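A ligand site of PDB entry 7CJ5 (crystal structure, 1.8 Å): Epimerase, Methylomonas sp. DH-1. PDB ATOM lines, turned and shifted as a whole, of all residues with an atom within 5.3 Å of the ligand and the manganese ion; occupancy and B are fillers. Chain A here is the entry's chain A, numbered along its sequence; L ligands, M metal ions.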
ATOM      1  N   HIS A  12      -0.205  25.414   7.679  1.00  0.00           N
ATOM      2  CA  HIS A  12       0.382  24.597   8.765  1.00  0.00           C
ATOM      3  C   HIS A  12      -0.093  25.156  10.105  1.00  0.00           C
ATOM      4  O   HIS A  12       0.073  26.372  10.326  1.00  0.00           O
ATOM      5  CB  HIS A  12       1.908  24.557   8.664  1.00  0.00           C
ATOM      6  CG  HIS A  12       2.513  23.416   9.404  1.00  0.00           C
ATOM      7  ND1 HIS A  12       2.458  23.327  10.785  1.00  0.00           N
ATOM      8  CD2 HIS A  12       3.189  22.325   8.981  1.00  0.00           C
ATOM      9  CE1 HIS A  12       3.085  22.242  11.177  1.00  0.00           C
ATOM     10  NE2 HIS A  12       3.542  21.595  10.086  1.00  0.00           N
ATOM     11  N   LEU A  14       1.121  25.157  12.900  1.00  0.00           N
ATOM     12  CA  LEU A  14       2.199  25.720  13.758  1.00  0.00           C
ATOM     13  C   LEU A  14       2.480  27.161  13.346  1.00  0.00           C
ATOM     14  O   LEU A  14       3.175  27.835  14.104  1.00  0.00           O
ATOM     15  CB  LEU A  14       3.465  24.863  13.644  1.00  0.00           C
ATOM     16  CG  LEU A  14       3.361  23.442  14.186  1.00  0.00           C
ATOM     17  CD1 LEU A  14       4.745  22.815  14.253  1.00  0.00           C
ATOM     18  CD2 LEU A  14       2.688  23.400  15.550  1.00  0.00           C
ATOM     19  N   GLU A  41      -3.214  21.798   8.118  1.00  0.00           N
ATOM     20  CA  GLU A  41      -2.284  20.667   8.357  1.00  0.00           C
ATOM     21  C   GLU A  41      -1.991  20.641   9.859  1.00  0.00           C
ATOM     22  O   GLU A  41      -1.298  21.543  10.370  1.00  0.00           O
ATOM     23  CB  GLU A  41      -1.026  20.819   7.525  1.00  0.00           C
ATOM     24  CG  GLU A  41      -0.098  19.629   7.654  1.00  0.00           C
ATOM     25  CD  GLU A  41       1.132  19.731   6.789  1.00  0.00           C
ATOM     26  OE1 GLU A  41       0.971  20.001   5.591  1.00  0.00           O
ATOM     27  OE2 GLU A  41       2.254  19.570   7.314  1.00  0.00           O
ATOM     28  N   ALA A  43      -0.323  19.400  13.258  1.00  0.00           N
ATOM     29  CA  ALA A  43       0.957  18.805  13.691  1.00  0.00           C
ATOM     30  C   ALA A  43       0.651  17.770  14.771  1.00  0.00           C
ATOM     31  O   ALA A  43       0.093  18.135  15.804  1.00  0.00           O
ATOM     32  CB  ALA A  43       1.883  19.894  14.177  1.00  0.00           C
ATOM     33  N   LEU A  45       2.791  15.634  16.424  1.00  0.00           N
ATOM     34  CA  LEU A  45       4.073  15.190  17.053  1.00  0.00           C
ATOM     35  C   LEU A  45       3.740  14.390  18.314  1.00  0.00           C
ATOM     36  O   LEU A  45       4.504  13.445  18.634  1.00  0.00           O
ATOM     37  CB  LEU A  45       4.962  16.397  17.346  1.00  0.00           C
ATOM     38  CG  LEU A  45       5.936  16.768  16.221  1.00  0.00           C
ATOM     39  CD1 LEU A  45       5.222  17.498  15.099  1.00  0.00           C
ATOM     40  CD2 LEU A  45       7.107  17.590  16.754  1.00  0.00           C
ATOM     41  N   SER A  69       0.602  16.187   9.621  1.00  0.00           N
ATOM     42  CA  SER A  69       2.051  15.917   9.485  1.00  0.00           C
ATOM     43  C   SER A  69       2.626  15.700  10.881  1.00  0.00           C
ATOM     44  O   SER A  69       2.012  16.147  11.885  1.00  0.00           O
ATOM     45  CB  SER A  69       2.760  17.040   8.765  1.00  0.00           C
ATOM     46  OG  SER A  69       2.660  18.254   9.484  1.00  0.00           O
ATOM     47  N   LEU A  70       3.757  15.035  10.944  1.00  0.00           N
ATOM     48  CA  LEU A  70       4.523  14.965  12.206  1.00  0.00           C
ATOM     49  C   LEU A  70       5.966  14.640  11.848  1.00  0.00           C
ATOM     50  O   LEU A  70       6.224  14.234  10.697  1.00  0.00           O
ATOM     51  CB  LEU A  70       3.914  13.901  13.120  1.00  0.00           C
ATOM     52  CG  LEU A  70       3.888  12.480  12.553  1.00  0.00           C
ATOM     53  CD1 LEU A  70       5.190  11.760  12.852  1.00  0.00           C
ATOM     54  CD2 LEU A  70       2.711  11.709  13.100  1.00  0.00           C
ATOM     55  N   GLY A  71       6.850  14.866  12.815  1.00  0.00           N
ATOM     56  CA  GLY A  71       8.198  14.296  12.856  1.00  0.00           C
ATOM     57  C   GLY A  71       8.328  13.411  14.081  1.00  0.00           C
ATOM     58  O   GLY A  71       7.808  13.796  15.149  1.00  0.00           O
ATOM     59  N   CYS A 109       1.553  13.124   6.288  1.00  0.00           N
ATOM     60  CA  CYS A 109       2.825  13.487   5.615  1.00  0.00           C
ATOM     61  C   CYS A 109       3.846  13.951   6.657  1.00  0.00           C
ATOM     62  O   CYS A 109       3.572  13.873   7.869  1.00  0.00           O
ATOM     63  CB  CYS A 109       2.593  14.554   4.560  1.00  0.00           C
ATOM     64  SG  CYS A 109       2.022  16.127   5.252  1.00  0.00           S
ATOM     65  N   GLY A 110       4.983  14.442   6.163  1.00  0.00           N
ATOM     66  CA  GLY A 110       6.073  14.940   7.010  1.00  0.00           C
ATOM     67  C   GLY A 110       7.137  13.885   7.252  1.00  0.00           C
ATOM     68  O   GLY A 110       7.252  12.930   6.440  1.00  0.00           O
ATOM     69  N   VAL A 111       7.914  14.063   8.318  1.00  0.00           N
ATOM     70  CA  VAL A 111       9.086  13.202   8.625  1.00  0.00           C
ATOM     71  C   VAL A 111       8.572  12.045   9.485  1.00  0.00           C
ATOM     72  O   VAL A 111       8.843  12.009  10.702  1.00  0.00           O
ATOM     73  CB  VAL A 111      10.232  14.033   9.237  1.00  0.00           C
ATOM     74  CG1 VAL A 111      11.504  13.207   9.424  1.00  0.00           C
ATOM     75  CG2 VAL A 111      10.533  15.246   8.377  1.00  0.00           C
ATOM     76  N   LEU A 116      13.038  13.538  13.381  1.00  0.00           N
ATOM     77  CA  LEU A 116      13.313  14.869  12.801  1.00  0.00           C
ATOM     78  C   LEU A 116      14.474  15.509  13.569  1.00  0.00           C
ATOM     79  O   LEU A 116      14.334  15.744  14.775  1.00  0.00           O
ATOM     80  CB  LEU A 116      12.050  15.735  12.895  1.00  0.00           C
ATOM     81  CG  LEU A 116      12.213  17.171  12.414  1.00  0.00           C
ATOM     82  CD1 LEU A 116      12.466  17.190  10.910  1.00  0.00           C
ATOM     83  CD2 LEU A 116      10.989  18.005  12.764  1.00  0.00           C
ATOM     84  N   GLU A 152       8.152  13.019   3.541  1.00  0.00           N
ATOM     85  CA  GLU A 152       8.720  14.367   3.313  1.00  0.00           C
ATOM     86  C   GLU A 152      10.244  14.287   3.258  1.00  0.00           C
ATOM     87  O   GLU A 152      10.864  14.065   4.304  1.00  0.00           O
ATOM     88  CB  GLU A 152       8.311  15.354   4.387  1.00  0.00           C
ATOM     89  CG  GLU A 152       8.629  16.782   3.986  1.00  0.00           C
ATOM     90  CD  GLU A 152       8.313  17.840   5.019  1.00  0.00           C
ATOM     91  OE1 GLU A 152       7.811  17.483   6.098  1.00  0.00           O
ATOM     92  OE2 GLU A 152       8.560  19.035   4.735  1.00  0.00           O
ATOM     93  N   VAL A 154      13.657  15.853   3.521  1.00  0.00           N
ATOM     94  CA  VAL A 154      14.153  17.060   4.238  1.00  0.00           C
ATOM     95  C   VAL A 154      15.672  17.108   4.130  1.00  0.00           C
ATOM     96  O   VAL A 154      16.296  16.111   3.689  1.00  0.00           O
ATOM     97  CB  VAL A 154      13.638  17.153   5.689  1.00  0.00           C
ATOM     98  CG1 VAL A 154      12.107  17.252   5.706  1.00  0.00           C
ATOM     99  CG2 VAL A 154      14.103  16.014   6.582  1.00  0.00           C
ATOM    100  N   GLU A 158      18.214  17.590   9.059  1.00  0.00           N
ATOM    101  CA  GLU A 158      16.906  17.178   9.630  1.00  0.00           C
ATOM    102  C   GLU A 158      16.619  15.692   9.389  1.00  0.00           C
ATOM    103  O   GLU A 158      15.703  15.174  10.069  1.00  0.00           O
ATOM    104  CB  GLU A 158      15.789  18.085   9.091  1.00  0.00           C
ATOM    105  CG  GLU A 158      15.951  19.529   9.539  1.00  0.00           C
ATOM    106  CD  GLU A 158      14.742  20.408   9.253  1.00  0.00           C
ATOM    107  OE1 GLU A 158      13.629  19.842   9.144  1.00  0.00           O
ATOM    108  OE2 GLU A 158      14.916  21.633   9.112  1.00  0.00           O
ATOM    109  N   HIS A 183       6.756  13.433  -0.779  1.00  0.00           N
ATOM    110  CA  HIS A 183       6.403  14.773  -0.267  1.00  0.00           C
ATOM    111  C   HIS A 183       7.643  15.660  -0.430  1.00  0.00           C
ATOM    112  O   HIS A 183       8.712  15.292   0.088  1.00  0.00           O
ATOM    113  CB  HIS A 183       5.835  14.605   1.140  1.00  0.00           C
ATOM    114  CG  HIS A 183       5.580  15.857   1.898  1.00  0.00           C
ATOM    115  ND1 HIS A 183       5.216  15.842   3.230  1.00  0.00           N
ATOM    116  CD2 HIS A 183       5.669  17.160   1.538  1.00  0.00           C
ATOM    117  CE1 HIS A 183       5.066  17.079   3.654  1.00  0.00           C
ATOM    118  NE2 HIS A 183       5.346  17.911   2.625  1.00  0.00           N
ATOM    119  N   ASP A 185       9.380  19.681  -0.340  1.00  0.00           N
ATOM    120  CA  ASP A 185       9.342  20.937   0.444  1.00  0.00           C
ATOM    121  C   ASP A 185      10.376  21.897  -0.150  1.00  0.00           C
ATOM    122  O   ASP A 185      11.564  21.538  -0.140  1.00  0.00           O
ATOM    123  CB  ASP A 185       9.635  20.634   1.919  1.00  0.00           C
ATOM    124  CG  ASP A 185       9.605  21.863   2.812  1.00  0.00           C
ATOM    125  OD1 ASP A 185      10.060  22.920   2.353  1.00  0.00           O
ATOM    126  OD2 ASP A 185       9.130  21.738   3.967  1.00  0.00           O
ATOM    127  N   TYR A 187      11.800  24.587   0.776  1.00  0.00           N
ATOM    128  CA  TYR A 187      12.876  25.034   1.711  1.00  0.00           C
ATOM    129  C   TYR A 187      14.014  23.997   1.693  1.00  0.00           C
ATOM    130  O   TYR A 187      15.200  24.362   1.574  1.00  0.00           O
ATOM    131  CB  TYR A 187      12.326  25.229   3.122  1.00  0.00           C
ATOM    132  CG  TYR A 187      13.379  25.291   4.206  1.00  0.00           C
ATOM    133  CD1 TYR A 187      14.127  26.439   4.419  1.00  0.00           C
ATOM    134  CD2 TYR A 187      13.624  24.191   5.007  1.00  0.00           C
ATOM    135  CE1 TYR A 187      15.089  26.491   5.429  1.00  0.00           C
ATOM    136  CE2 TYR A 187      14.588  24.223   6.004  1.00  0.00           C
ATOM    137  CZ  TYR A 187      15.316  25.380   6.222  1.00  0.00           C
ATOM    138  OH  TYR A 187      16.263  25.417   7.202  1.00  0.00           O
ATOM    139  N   HIS A 188      13.654  22.727   1.805  1.00  0.00           N
ATOM    140  CA  HIS A 188      14.624  21.596   1.799  1.00  0.00           C
ATOM    141  C   HIS A 188      15.233  21.457   0.394  1.00  0.00           C
ATOM    142  O   HIS A 188      16.457  21.278   0.287  1.00  0.00           O
ATOM    143  CB  HIS A 188      13.930  20.329   2.301  1.00  0.00           C
ATOM    144  CG  HIS A 188      13.485  20.459   3.721  1.00  0.00           C
ATOM    145  ND1 HIS A 188      14.381  20.741   4.745  1.00  0.00           N
ATOM    146  CD2 HIS A 188      12.264  20.372   4.297  1.00  0.00           C
ATOM    147  CE1 HIS A 188      13.736  20.796   5.899  1.00  0.00           C
ATOM    148  NE2 HIS A 188      12.432  20.594   5.642  1.00  0.00           N
ATOM    149  N   HIS A 211       5.076  21.013   0.428  1.00  0.00           N
ATOM    150  CA  HIS A 211       5.272  22.142   1.373  1.00  0.00           C
ATOM    151  C   HIS A 211       5.938  23.302   0.635  1.00  0.00           C
ATOM    152  O   HIS A 211       6.925  23.083  -0.087  1.00  0.00           O
ATOM    153  CB  HIS A 211       6.097  21.718   2.585  1.00  0.00           C
ATOM    154  CG  HIS A 211       5.292  21.011   3.619  1.00  0.00           C
ATOM    155  ND1 HIS A 211       5.833  20.585   4.798  1.00  0.00           N
ATOM    156  CD2 HIS A 211       3.986  20.657   3.651  1.00  0.00           C
ATOM    157  CE1 HIS A 211       4.913  19.999   5.521  1.00  0.00           C
ATOM    158  NE2 HIS A 211       3.760  20.016   4.829  1.00  0.00           N
ATOM    159  N   ARG A 217      12.690  30.502   5.350  1.00  0.00           N
ATOM    160  CA  ARG A 217      11.357  30.142   5.944  1.00  0.00           C
ATOM    161  C   ARG A 217      10.565  31.392   6.361  1.00  0.00           C
ATOM    162  O   ARG A 217       9.610  31.261   7.164  1.00  0.00           O
ATOM    163  CB  ARG A 217      11.489  29.220   7.163  1.00  0.00           C
ATOM    164  CG  ARG A 217      12.577  28.166   7.029  1.00  0.00           C
ATOM    165  CD  ARG A 217      12.342  26.973   7.950  1.00  0.00           C
ATOM    166  NE  ARG A 217      11.508  25.975   7.312  1.00  0.00           N
ATOM    167  CZ  ARG A 217      11.485  24.696   7.629  1.00  0.00           C
ATOM    168  NH1 ARG A 217      12.241  24.249   8.606  1.00  0.00           N
ATOM    169  NH2 ARG A 217      10.706  23.866   6.961  1.00  0.00           N
ATOM    170  N   GLU A 246       4.117  26.758   5.194  1.00  0.00           N
ATOM    171  CA  GLU A 246       4.570  26.663   6.601  1.00  0.00           C
ATOM    172  C   GLU A 246       5.752  27.598   6.869  1.00  0.00           C
ATOM    173  O   GLU A 246       6.538  27.908   5.940  1.00  0.00           O
ATOM    174  CB  GLU A 246       4.938  25.219   6.917  1.00  0.00           C
ATOM    175  CG  GLU A 246       6.226  24.780   6.277  1.00  0.00           C
ATOM    176  CD  GLU A 246       6.555  23.322   6.497  1.00  0.00           C
ATOM    177  OE1 GLU A 246       5.873  22.673   7.306  1.00  0.00           O
ATOM    178  OE2 GLU A 246       7.484  22.846   5.835  1.00  0.00           O
ATOM    179  N   PHE A 248       7.933  28.809  10.982  1.00  0.00           N
ATOM    180  CA  PHE A 248       8.088  28.366  12.395  1.00  0.00           C
ATOM    181  C   PHE A 248       8.701  29.504  13.212  1.00  0.00           C
ATOM    182  O   PHE A 248       9.910  29.699  13.117  1.00  0.00           O
ATOM    183  CB  PHE A 248       8.941  27.096  12.426  1.00  0.00           C
ATOM    184  CG  PHE A 248       8.349  25.994  11.589  1.00  0.00           C
ATOM    185  CD1 PHE A 248       7.262  25.277  12.052  1.00  0.00           C
ATOM    186  CD2 PHE A 248       8.835  25.705  10.324  1.00  0.00           C
ATOM    187  CE1 PHE A 248       6.683  24.280  11.288  1.00  0.00           C
ATOM    188  CE2 PHE A 248       8.254  24.710   9.550  1.00  0.00           C
ATOM    189  CZ  PHE A 248       7.178  23.997  10.033  1.00  0.00           C
ATOM    190  N   LEU A 261      14.755  22.944  14.590  1.00  0.00           N
ATOM    191  CA  LEU A 261      14.736  23.632  13.274  1.00  0.00           C
ATOM    192  C   LEU A 261      15.735  24.810  13.293  1.00  0.00           C
ATOM    193  O   LEU A 261      15.920  25.451  12.226  1.00  0.00           O
ATOM    194  CB  LEU A 261      13.315  24.100  12.987  1.00  0.00           C
ATOM    195  CG  LEU A 261      12.291  22.983  12.827  1.00  0.00           C
ATOM    196  CD1 LEU A 261      10.935  23.529  12.403  1.00  0.00           C
ATOM    197  CD2 LEU A 261      12.778  21.942  11.832  1.00  0.00           C
HETATM  198  C1  LIG L   1      10.566  20.715   9.042  1.00  0.00           C
HETATM  199  C2  LIG L   1       9.461  20.726   8.019  1.00  0.00           C
HETATM  200  C3  LIG L   1       8.055  20.473   8.498  1.00  0.00           C
HETATM  201  C4  LIG L   1       8.184  19.257   9.390  1.00  0.00           C
HETATM  202  C5  LIG L   1       6.984  18.877  10.263  1.00  0.00           C
HETATM  203  C6  LIG L   1       5.802  19.819  10.227  1.00  0.00           C
HETATM  204  O1  LIG L   1      11.720  21.391   8.538  1.00  0.00           O
HETATM  205  O2  LIG L   1       9.717  20.961   6.842  1.00  0.00           O
HETATM  206  O3  LIG L   1       7.175  20.226   7.394  1.00  0.00           O
HETATM  207  O4  LIG L   1       8.521  18.209   8.509  1.00  0.00           O
HETATM  208  O5  LIG L   1       6.599  17.539   9.969  1.00  0.00           O
HETATM  209  O6  LIG L   1       4.810  19.299  11.150  1.00  0.00           O
HETATM  210 MN    MN M   1       8.010  20.851   5.404  1.00  0.00          MN
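The backbone carbonyl oxygen of Leu 70 lies within hydrogen-bond range of an oxygen (O5) of the ligand (3.4 Å).
An oxygen (O1) of the ligand lies within hydrogen-bond range of a ring nitrogen (NE2) of His 188, 3.1 Å away.
An oxygen (O6) of the ligand lies within hydrogen-bond range of the side-chain hydroxyl of Ser 69, 2.9 Å away.
NE2 of His 12 is in hydrogen-bond range of O6 of the ligand, 2.8 Å away.
The side-chain carboxylate (OE1) of Glu 158 is in hydrogen-bond range of an oxygen (O1) of the ligand, at 2.5 Å.
O1 of the ligand lies within hydrogen-bond range of NH1 of Arg 217 (2.9 Å).
ND1 of His 183 sits at hydrogen-bond distance from N of Gly 110 (3.3 Å).
NE2 of His 211 is in hydrogen-bond range of OE1 of Glu 41 (2.9 Å).
The side-chain carboxylate (OE2) of Glu 41 sits at hydrogen-bond distance from the side-chain hydroxyl (OG) of Ser 69 (2.6 Å).
OD1 of Asp 185 lies within hydrogen-bond range of N of Tyr 187 (2.9 Å).
The backbone carbonyl oxygen (O) of Leu 70 sits at hydrogen-bond distance from the backbone NH (N) of Val 111 (2.9 Å).
O of Gly 110 sits at hydrogen-bond distance from N of Glu 152 (3.0 Å).
A ring nitrogen (NE2) of His 183 lies close to a ring nitrogen (NE2) of His 211 (3.4 Å).
The side-chain carboxylate (OE2) of Glu 246 lies close to the guanidinium group (NH2) of Arg 217.
Merely in contact with the ligand: Leu 261 (3.5 Å), Val 111 (3.6 Å), Gly 71 (3.9 Å), Phe 248 (3.9 Å) and Gly 110 (3.97 Å).
Hydrophobic or aromatic side chains that line the ligand: His 12, Val 111, His 188, His 211, Phe 248 and Leu 261.
15 residues have an atom within 4 Å of the ligand: His 12, Ser 69, Leu 70, Gly 71, Gly 110, Val 111, Glu 152, Glu 158, Asp 185, His 188, His 211, Arg 217, Glu 246, Phe 248 and Leu 261.
The nearest printed residue that does not touch the ligand is Ala 43 (4.3 Å).
Four residues have an atom within 4 Å of the manganese ion: Glu 152, Asp 185, His 211 and Glu 246.
The nearest printed residue that does not touch the manganese ion is Arg 217 (4.3 Å).
The side-chain carboxylate (OE2) of Glu 152 is bound to the manganese ion (2.0 Å).
OD2 of Asp 185 is bound to the manganese ion (2.0 Å).
The side-chain carboxylate (OE2) of Glu 246 binds the manganese ion.
O2 of the ligand is bound to the manganese ion, 2.2 Å away.
An oxygen (O3) of the ligand is bound to the manganese ion, at 2.2 Å.
A ring nitrogen (ND1) of His 211 is bound to the manganese ion, 2.3 Å away.
The manganese ion has six donor atoms within binding distance.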
